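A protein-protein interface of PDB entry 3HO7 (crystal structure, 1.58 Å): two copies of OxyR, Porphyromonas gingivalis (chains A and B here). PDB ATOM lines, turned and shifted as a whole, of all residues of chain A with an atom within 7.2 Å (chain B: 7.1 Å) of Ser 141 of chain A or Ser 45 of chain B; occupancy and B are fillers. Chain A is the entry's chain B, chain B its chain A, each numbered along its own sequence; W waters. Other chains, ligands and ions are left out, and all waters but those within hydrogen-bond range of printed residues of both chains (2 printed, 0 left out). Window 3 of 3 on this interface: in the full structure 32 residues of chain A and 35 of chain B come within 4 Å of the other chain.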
ATOM      1  N   TRP A 112      13.100  -7.645 -24.417  1.00  0.00           N
ATOM      2  CA  TRP A 112      11.822  -7.746 -25.112  1.00  0.00           C
ATOM      3  C   TRP A 112      11.689  -6.595 -26.101  1.00  0.00           C
ATOM      4  O   TRP A 112      11.618  -5.433 -25.702  1.00  0.00           O
ATOM      5  CB  TRP A 112      10.655  -7.711 -24.122  1.00  0.00           C
ATOM      6  CG  TRP A 112      10.762  -8.705 -23.012  1.00  0.00           C
ATOM      7  CD1 TRP A 112      11.020  -8.438 -21.700  1.00  0.00           C
ATOM      8  CD2 TRP A 112      10.613 -10.128 -23.110  1.00  0.00           C
ATOM      9  NE1 TRP A 112      11.042  -9.605 -20.975  1.00  0.00           N
ATOM     10  CE2 TRP A 112      10.795 -10.657 -21.817  1.00  0.00           C
ATOM     11  CE3 TRP A 112      10.345 -11.006 -24.165  1.00  0.00           C
ATOM     12  CZ2 TRP A 112      10.717 -12.021 -21.551  1.00  0.00           C
ATOM     13  CZ3 TRP A 112      10.268 -12.362 -23.899  1.00  0.00           C
ATOM     14  CH2 TRP A 112      10.454 -12.855 -22.603  1.00  0.00           C
ATOM     15  N   LEU A 113      11.640  -6.926 -27.388  1.00  0.00           N
ATOM     16  CA  LEU A 113      11.554  -5.926 -28.450  1.00  0.00           C
ATOM     17  C   LEU A 113      10.248  -6.007 -29.238  1.00  0.00           C
ATOM     18  O   LEU A 113       9.781  -7.090 -29.576  1.00  0.00           O
ATOM     19  CB  LEU A 113      12.737  -6.059 -29.410  1.00  0.00           C
ATOM     20  CG  LEU A 113      14.110  -5.632 -28.891  1.00  0.00           C
ATOM     21  CD1 LEU A 113      15.175  -5.866 -29.950  1.00  0.00           C
ATOM     22  CD2 LEU A 113      14.091  -4.179 -28.455  1.00  0.00           C
ATOM     23  N   ASP A 115       7.941  -5.619 -32.511  1.00  0.00           N
ATOM     24  CA  ASP A 115       8.098  -5.770 -33.957  1.00  0.00           C
ATOM     25  C   ASP A 115       8.207  -4.426 -34.678  1.00  0.00           C
ATOM     26  O   ASP A 115       9.149  -4.191 -35.436  1.00  0.00           O
ATOM     27  CB  ASP A 115       6.937  -6.586 -34.530  1.00  0.00           C
ATOM     28  CG  ASP A 115       6.818  -7.956 -33.890  1.00  0.00           C
ATOM     29  OD1 ASP A 115       7.749  -8.347 -33.154  1.00  0.00           O
ATOM     30  OD2 ASP A 115       5.798  -8.641 -34.119  1.00  0.00           O
ATOM     31  N   THR A 138      12.437 -18.768 -24.943  1.00  0.00           N
ATOM     32  CA  THR A 138      11.149 -18.230 -25.357  1.00  0.00           C
ATOM     33  C   THR A 138      11.281 -17.026 -26.282  1.00  0.00           C
ATOM     34  O   THR A 138      11.594 -15.920 -25.839  1.00  0.00           O
ATOM     35  CB  THR A 138      10.300 -17.819 -24.140  1.00  0.00           C
ATOM     36  OG1 THR A 138      10.070 -18.962 -23.308  1.00  0.00           O
ATOM     37  CG2 THR A 138       8.968 -17.246 -24.593  1.00  0.00           C
ATOM     38  N   ALA A 139      11.037 -17.247 -27.569  1.00  0.00           N
ATOM     39  CA  ALA A 139      10.969 -16.158 -28.532  1.00  0.00           C
ATOM     40  C   ALA A 139       9.571 -15.553 -28.500  1.00  0.00           C
ATOM     41  O   ALA A 139       8.582 -16.242 -28.749  1.00  0.00           O
ATOM     42  CB  ALA A 139      11.298 -16.662 -29.926  1.00  0.00           C
ATOM     43  N   TYR A 140       9.490 -14.265 -28.187  1.00  0.00           N
ATOM     44  CA  TYR A 140       8.200 -13.596 -28.078  1.00  0.00           C
ATOM     45  C   TYR A 140       7.902 -12.791 -29.337  1.00  0.00           C
ATOM     46  O   TYR A 140       8.498 -11.740 -29.568  1.00  0.00           O
ATOM     47  CB  TYR A 140       8.172 -12.684 -26.853  1.00  0.00           C
ATOM     48  CG  TYR A 140       6.781 -12.396 -26.337  1.00  0.00           C
ATOM     49  CD1 TYR A 140       5.682 -12.438 -27.185  1.00  0.00           C
ATOM     50  CD2 TYR A 140       6.570 -12.068 -25.005  1.00  0.00           C
ATOM     51  CE1 TYR A 140       4.410 -12.170 -26.717  1.00  0.00           C
ATOM     52  CE2 TYR A 140       5.302 -11.797 -24.530  1.00  0.00           C
ATOM     53  CZ  TYR A 140       4.226 -11.851 -25.389  1.00  0.00           C
ATOM     54  OH  TYR A 140       2.964 -11.580 -24.917  1.00  0.00           O
ATOM     55  N   SER A 141       6.972 -13.290 -30.145  1.00  0.00           N
ATOM     56  CA  SER A 141       6.632 -12.646 -31.408  1.00  0.00           C
ATOM     57  C   SER A 141       5.408 -11.741 -31.290  1.00  0.00           C
ATOM     58  O   SER A 141       4.389 -12.123 -30.714  1.00  0.00           O
ATOM     59  CB  SER A 141       6.406 -13.698 -32.497  1.00  0.00           C
ATOM     60  OG  SER A 141       6.087 -13.091 -33.737  1.00  0.00           O
ATOM     61  N   GLY A 142       5.519 -10.539 -31.847  1.00  0.00           N
ATOM     62  CA  GLY A 142       4.409  -9.595 -31.874  1.00  0.00           C
ATOM     63  C   GLY A 142       3.744  -9.426 -30.525  1.00  0.00           C
ATOM     64  O   GLY A 142       2.517  -9.455 -30.419  1.00  0.00           O
ATOM     65  N   GLY A 143       4.554  -9.256 -29.487  1.00  0.00           N
ATOM     66  CA  GLY A 143       4.036  -9.021 -28.147  1.00  0.00           C
ATOM     67  C   GLY A 143       3.534  -7.598 -28.006  1.00  0.00           C
ATOM     68  O   GLY A 143       3.882  -6.724 -28.804  1.00  0.00           O
ATOM     69  N   SER A 144       2.705  -7.361 -26.994  1.00  0.00           N
ATOM     70  CA  SER A 144       2.194  -6.021 -26.734  1.00  0.00           C
ATOM     71  C   SER A 144       3.084  -5.292 -25.736  1.00  0.00           C
ATOM     72  O   SER A 144       3.795  -5.921 -24.949  1.00  0.00           O
ATOM     73  CB  SER A 144       0.755  -6.080 -26.209  1.00  0.00           C
ATOM     74  OG  SER A 144       0.694  -6.658 -24.913  1.00  0.00           O
ATOM     75  N   PHE A 148       5.071  -6.918 -22.294  1.00  0.00           N
ATOM     76  CA  PHE A 148       6.478  -6.666 -21.994  1.00  0.00           C
ATOM     77  C   PHE A 148       6.651  -5.885 -20.693  1.00  0.00           C
ATOM     78  O   PHE A 148       7.540  -6.181 -19.896  1.00  0.00           O
ATOM     79  CB  PHE A 148       7.164  -5.929 -23.150  1.00  0.00           C
ATOM     80  CG  PHE A 148       7.342  -6.767 -24.384  1.00  0.00           C
ATOM     81  CD1 PHE A 148       6.966  -8.099 -24.391  1.00  0.00           C
ATOM     82  CD2 PHE A 148       7.913  -6.233 -25.526  1.00  0.00           C
ATOM     83  CE1 PHE A 148       7.133  -8.877 -25.523  1.00  0.00           C
ATOM     84  CE2 PHE A 148       8.087  -7.011 -26.662  1.00  0.00           C
ATOM     85  CZ  PHE A 148       7.697  -8.331 -26.657  1.00  0.00           C
ATOM     86  N   ASN B  14       5.631 -23.720 -31.018  1.00  0.00           N
ATOM     87  CA  ASN B  14       5.064 -22.451 -31.457  1.00  0.00           C
ATOM     88  C   ASN B  14       3.665 -22.270 -30.886  1.00  0.00           C
ATOM     89  O   ASN B  14       2.729 -22.944 -31.308  1.00  0.00           O
ATOM     90  CB  ASN B  14       5.015 -22.389 -32.982  1.00  0.00           C
ATOM     91  CG  ASN B  14       6.359 -22.678 -33.620  1.00  0.00           C
ATOM     92  OD1 ASN B  14       7.389 -22.163 -33.183  1.00  0.00           O
ATOM     93  ND2 ASN B  14       6.356 -23.506 -34.660  1.00  0.00           N
ATOM     94  N   ILE B  15       3.527 -21.361 -29.927  1.00  0.00           N
ATOM     95  CA  ILE B  15       2.247 -21.164 -29.256  1.00  0.00           C
ATOM     96  C   ILE B  15       1.746 -19.727 -29.346  1.00  0.00           C
ATOM     97  O   ILE B  15       2.486 -18.776 -29.094  1.00  0.00           O
ATOM     98  CB  ILE B  15       2.315 -21.581 -27.777  1.00  0.00           C
ATOM     99  CG1 ILE B  15       0.964 -21.344 -27.099  1.00  0.00           C
ATOM    100  CG2 ILE B  15       3.420 -20.823 -27.060  1.00  0.00           C
ATOM    101  CD1 ILE B  15       0.948 -21.696 -25.634  1.00  0.00           C
ATOM    102  N   ALA B  16       0.475 -19.580 -29.706  1.00  0.00           N
ATOM    103  CA  ALA B  16      -0.148 -18.272 -29.791  1.00  0.00           C
ATOM    104  C   ALA B  16      -0.889 -17.967 -28.497  1.00  0.00           C
ATOM    105  O   ALA B  16      -1.267 -18.874 -27.754  1.00  0.00           O
ATOM    106  CB  ALA B  16      -1.099 -18.211 -30.974  1.00  0.00           C
ATOM    107  N   VAL B  17      -1.088 -16.684 -28.228  1.00  0.00           N
ATOM    108  CA  VAL B  17      -1.792 -16.261 -27.032  1.00  0.00           C
ATOM    109  C   VAL B  17      -2.585 -15.002 -27.329  1.00  0.00           C
ATOM    110  O   VAL B  17      -2.119 -14.120 -28.051  1.00  0.00           O
ATOM    111  CB  VAL B  17      -0.815 -15.986 -25.872  1.00  0.00           C
ATOM    112  CG1 VAL B  17      -1.579 -15.656 -24.597  1.00  0.00           C
ATOM    113  CG2 VAL B  17       0.101 -17.181 -25.662  1.00  0.00           C
ATOM    114  N   LEU B  18      -3.791 -14.925 -26.778  1.00  0.00           N
ATOM    115  CA  LEU B  18      -4.619 -13.742 -26.944  1.00  0.00           C
ATOM    116  C   LEU B  18      -3.986 -12.524 -26.291  1.00  0.00           C
ATOM    117  O   LEU B  18      -3.308 -12.634 -25.268  1.00  0.00           O
ATOM    118  CB  LEU B  18      -6.019 -13.973 -26.376  1.00  0.00           C
ATOM    119  CG  LEU B  18      -6.975 -14.733 -27.297  1.00  0.00           C
ATOM    120  CD1 LEU B  18      -6.332 -16.018 -27.790  1.00  0.00           C
ATOM    121  CD2 LEU B  18      -8.296 -15.010 -26.591  1.00  0.00           C
ATOM    122  N   ALA B  22      -2.225 -12.655 -22.752  1.00  0.00           N
ATOM    123  CA  ALA B  22      -0.762 -12.636 -22.728  1.00  0.00           C
ATOM    124  C   ALA B  22      -0.150 -11.894 -21.543  1.00  0.00           C
ATOM    125  O   ALA B  22       0.732 -12.425 -20.865  1.00  0.00           O
ATOM    126  CB  ALA B  22      -0.226 -12.073 -24.035  1.00  0.00           C
ATOM    127  N   LEU B  26       1.238 -14.832 -19.061  1.00  0.00           N
ATOM    128  CA  LEU B  26       2.622 -15.157 -19.395  1.00  0.00           C
ATOM    129  C   LEU B  26       3.633 -14.786 -18.307  1.00  0.00           C
ATOM    130  O   LEU B  26       4.557 -15.550 -18.031  1.00  0.00           O
ATOM    131  CB  LEU B  26       3.009 -14.555 -20.749  1.00  0.00           C
ATOM    132  CG  LEU B  26       2.168 -15.102 -21.907  1.00  0.00           C
ATOM    133  CD1 LEU B  26       2.634 -14.524 -23.233  1.00  0.00           C
ATOM    134  CD2 LEU B  26       2.202 -16.626 -21.936  1.00  0.00           C
ATOM    135  N   HIS B  43       8.412 -20.539 -29.129  1.00  0.00           N
ATOM    136  CA  HIS B  43       8.097 -19.321 -29.863  1.00  0.00           C
ATOM    137  C   HIS B  43       6.694 -18.832 -29.526  1.00  0.00           C
ATOM    138  O   HIS B  43       5.705 -19.399 -29.984  1.00  0.00           O
ATOM    139  CB  HIS B  43       8.226 -19.547 -31.370  1.00  0.00           C
ATOM    140  CG  HIS B  43       9.633 -19.466 -31.873  1.00  0.00           C
ATOM    141  ND1 HIS B  43      10.551 -20.476 -31.685  1.00  0.00           N
ATOM    142  CD2 HIS B  43      10.277 -18.493 -32.561  1.00  0.00           C
ATOM    143  CE1 HIS B  43      11.702 -20.129 -32.232  1.00  0.00           C
ATOM    144  NE2 HIS B  43      11.563 -18.931 -32.772  1.00  0.00           N
ATOM    145  N   VAL B  44       6.620 -17.781 -28.716  1.00  0.00           N
ATOM    146  CA  VAL B  44       5.343 -17.197 -28.331  1.00  0.00           C
ATOM    147  C   VAL B  44       4.921 -16.128 -29.327  1.00  0.00           C
ATOM    148  O   VAL B  44       5.748 -15.350 -29.804  1.00  0.00           O
ATOM    149  CB  VAL B  44       5.417 -16.553 -26.938  1.00  0.00           C
ATOM    150  CG1 VAL B  44       4.108 -15.845 -26.611  1.00  0.00           C
ATOM    151  CG2 VAL B  44       5.749 -17.600 -25.886  1.00  0.00           C
ATOM    152  N   SER B  45       3.631 -16.092 -29.639  1.00  0.00           N
ATOM    153  CA  SER B  45       3.091 -15.065 -30.518  1.00  0.00           C
ATOM    154  C   SER B  45       1.689 -14.669 -30.075  1.00  0.00           C
ATOM    155  O   SER B  45       0.877 -15.524 -29.722  1.00  0.00           O
ATOM    156  CB  SER B  45       3.071 -15.554 -31.967  1.00  0.00           C
ATOM    157  OG  SER B  45       2.338 -16.760 -32.086  1.00  0.00           O
ATOM    158  N   GLU B  46       1.415 -13.369 -30.082  1.00  0.00           N
ATOM    159  CA  GLU B  46       0.084 -12.873 -29.768  1.00  0.00           C
ATOM    160  C   GLU B  46      -0.755 -12.771 -31.037  1.00  0.00           C
ATOM    161  O   GLU B  46      -0.338 -12.169 -32.026  1.00  0.00           O
ATOM    162  CB  GLU B  46       0.152 -11.509 -29.073  1.00  0.00           C
ATOM    163  CG  GLU B  46       0.758 -11.542 -27.677  1.00  0.00           C
ATOM    164  CD  GLU B  46       0.599 -10.227 -26.934  1.00  0.00           C
ATOM    165  OE1 GLU B  46      -0.476  -9.596 -27.042  1.00  0.00           O
ATOM    166  OE2 GLU B  46       1.552  -9.824 -26.234  1.00  0.00           O
ATOM    167  N   MET B  47      -1.935 -13.380 -30.997  1.00  0.00           N
ATOM    168  CA  MET B  47      -2.899 -13.283 -32.084  1.00  0.00           C
ATOM    169  C   MET B  47      -4.290 -13.195 -31.491  1.00  0.00           C
ATOM    170  O   MET B  47      -4.529 -13.671 -30.382  1.00  0.00           O
ATOM    171  CB  MET B  47      -2.864 -14.529 -32.962  1.00  0.00           C
ATOM    172  CG  MET B  47      -1.511 -14.936 -33.487  1.00  0.00           C
ATOM    173  SD  MET B  47      -1.689 -16.493 -34.374  1.00  0.00           S
ATOM    174  CE  MET B  47       0.008 -16.806 -34.852  1.00  0.00           C
ATOM    175  N   CYS B  52      -5.441 -17.381 -34.498  1.00  0.00           N
ATOM    176  CA  CYS B  52      -5.117 -18.589 -33.747  1.00  0.00           C
ATOM    177  C   CYS B  52      -5.690 -19.831 -34.414  1.00  0.00           C
ATOM    178  O   CYS B  52      -4.974 -20.798 -34.666  1.00  0.00           O
ATOM    179  CB  CYS B  52      -5.644 -18.497 -32.315  1.00  0.00           C
ATOM    180  SG  CYS B  52      -4.733 -17.372 -31.244  1.00  0.00           S
ATOM    181  N   SER B  55      -4.100 -20.408 -37.848  1.00  0.00           N
ATOM    182  CA  SER B  55      -2.716 -20.854 -37.729  1.00  0.00           C
ATOM    183  C   SER B  55      -2.635 -22.298 -37.247  1.00  0.00           C
ATOM    184  O   SER B  55      -1.822 -23.079 -37.737  1.00  0.00           O
ATOM    185  CB  SER B  55      -1.932 -19.926 -36.802  1.00  0.00           C
ATOM    186  OG  SER B  55      -1.794 -18.642 -37.385  1.00  0.00           O
ATOM    187  N   GLU B  60       0.883 -23.394 -38.654  1.00  0.00           N
ATOM    188  CA  GLU B  60       1.771 -22.274 -38.354  1.00  0.00           C
ATOM    189  C   GLU B  60       2.125 -22.251 -36.871  1.00  0.00           C
ATOM    190  O   GLU B  60       3.198 -21.787 -36.483  1.00  0.00           O
ATOM    191  CB  GLU B  60       1.114 -20.951 -38.755  1.00  0.00           C
ATOM    192  CG  GLU B  60       1.970 -19.719 -38.485  1.00  0.00           C
ATOM    193  CD  GLU B  60       1.260 -18.421 -38.842  1.00  0.00           C
ATOM    194  OE1 GLU B  60       0.155 -18.484 -39.420  1.00  0.00           O
ATOM    195  OE2 GLU B  60       1.809 -17.339 -38.545  1.00  0.00           O
ATOM    196  N   ILE B  61       1.211 -22.751 -36.045  1.00  0.00           N
ATOM    197  CA  ILE B  61       1.433 -22.829 -34.605  1.00  0.00           C
ATOM    198  C   ILE B  61       0.959 -24.174 -34.063  1.00  0.00           C
ATOM    199  O   ILE B  61       0.038 -24.782 -34.609  1.00  0.00           O
ATOM    200  CB  ILE B  61       0.720 -21.685 -33.854  1.00  0.00           C
ATOM    201  CG1 ILE B  61      -0.800 -21.870 -33.898  1.00  0.00           C
ATOM    202  CG2 ILE B  61       1.119 -20.337 -34.435  1.00  0.00           C
ATOM    203  CD1 ILE B  61      -1.565 -20.795 -33.147  1.00  0.00           C
ATOM    204  N   MET B  63       0.025 -24.818 -30.679  1.00  0.00           N
ATOM    205  CA  MET B  63      -1.031 -24.665 -29.686  1.00  0.00           C
ATOM    206  C   MET B  63      -1.479 -23.215 -29.627  1.00  0.00           C
ATOM    207  O   MET B  63      -0.759 -22.313 -30.057  1.00  0.00           O
ATOM    208  CB  MET B  63      -0.539 -25.104 -28.305  1.00  0.00           C
ATOM    209  CG  MET B  63       0.160 -26.451 -28.286  1.00  0.00           C
ATOM    210  SD  MET B  63       0.856 -26.871 -26.674  1.00  0.00           S
ATOM    211  CE  MET B  63       1.571 -28.473 -27.048  1.00  0.00           C
HETATM  212  O   HOH W   1      -0.472  -7.987 -29.552  1.00  0.00           O
HETATM  213  O   HOH W   2      -1.423  -8.058 -25.384  1.00  0.00           O
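N of Val 44 of chain B lies within hydrogen-bond range of O of Ala 139 of chain A (2.5 Å). O of Val 44 of chain B sits at hydrogen-bond distance from N of Ser 141 of chain A. OE2 of Glu 46 of chain B is in hydrogen-bond range of OH of Tyr 140 of chain A, at 2.6 Å. The backbone NH (N) of Glu 46 of chain B is in hydrogen-bond range of the backbone carbonyl oxygen (O) of Ser 141 of chain A, at 3.3 Å. N of Ser 144 of chain A is in hydrogen-bond range of OE2 of Glu 46 of chain B, 2.8 Å away.
Of chain B, only Val 44, Ser 45 and Glu 46 come within 4 Å of Ser 141 of chain A. Of the printed residues of chain B, Gly 143 of chain A touches Glu 46 (3.2 Å). Ser 45 of chain B touches just one residue of chain A: Ser 141. Of the printed residues of chain A, Glu 46 of chain B touches Tyr 140 (2.6 Å), Ser 141 (3.3 Å), Gly 142 (3.4 Å), Gly 143 (3.2 Å) and Ser 144 (2.8 Å). The nearest residue of chain B that does not touch Ser 141 of chain A is His 43 of chain B (5.6 Å). The nearest printed residue of chain A that does not touch Glu 46 of chain B is Phe 148 of chain A (5.7 Å).
The backbone carbonyl oxygen (O) of His 43 of chain B lies within hydrogen-bond range of the backbone NH (N) of Ile 15 of chain B, 2.9 Å away. The backbone NH of Ser 45 of chain B sits at hydrogen-bond distance from the backbone carbonyl oxygen of Ile 15 of chain B, 3.0 Å away. N of Val 17 of chain B is in hydrogen-bond range of O of Ser 45 of chain B, 2.7 Å away. The side-chain carboxylate (OD2) of Asp 115 of chain A lies close to the backbone NH (N) of Gly 142 of chain A, 3.0 Å away.
Along chain B the printed residues that touch a printed residue of chain A span positions 22 to 46. Of the 11 printed residues of chain A, 7 touch a printed residue of chain B.
Water W2 lies within hydrogen-bond range of the side-chain carboxylate of Glu 46 of chain B (2.5 Å) and the side-chain hydroxyl of Ser 144 of chain A (2.6 Å). Water W1 bridges OE1 of Glu 46 of chain B (3.0 Å) and O of Gly 142 of chain A (3.4 Å).
No position is printed for both chains. Of the 13 pairs that touch across the chains among the printed residues, none has its exchanged pair printed and touching as well.
CG2 of Val 44 of chain B touches CG2 of Thr 138 of chain A, 3.5 Å away. His 43 of chain B touches Ala 139 of chain A. Tyr 140 of chain A touches Ala 22 of chain B (OH to CB, 3.3 Å). OH of Tyr 140 of chain A touches CD1 of Leu 26 of chain B, 3.4 Å away. C of Tyr 140 of chain A touches O of Val 44 of chain B, 3.4 Å away. O of Ser 141 of chain A touches CA of Ser 45 of chain B, at 3.2 Å. Gly 142 of chain A touches Glu 46 of chain B. Glu 46 of chain B touches Gly 143 of chain A (OE2 to CA, 3.2 Å).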
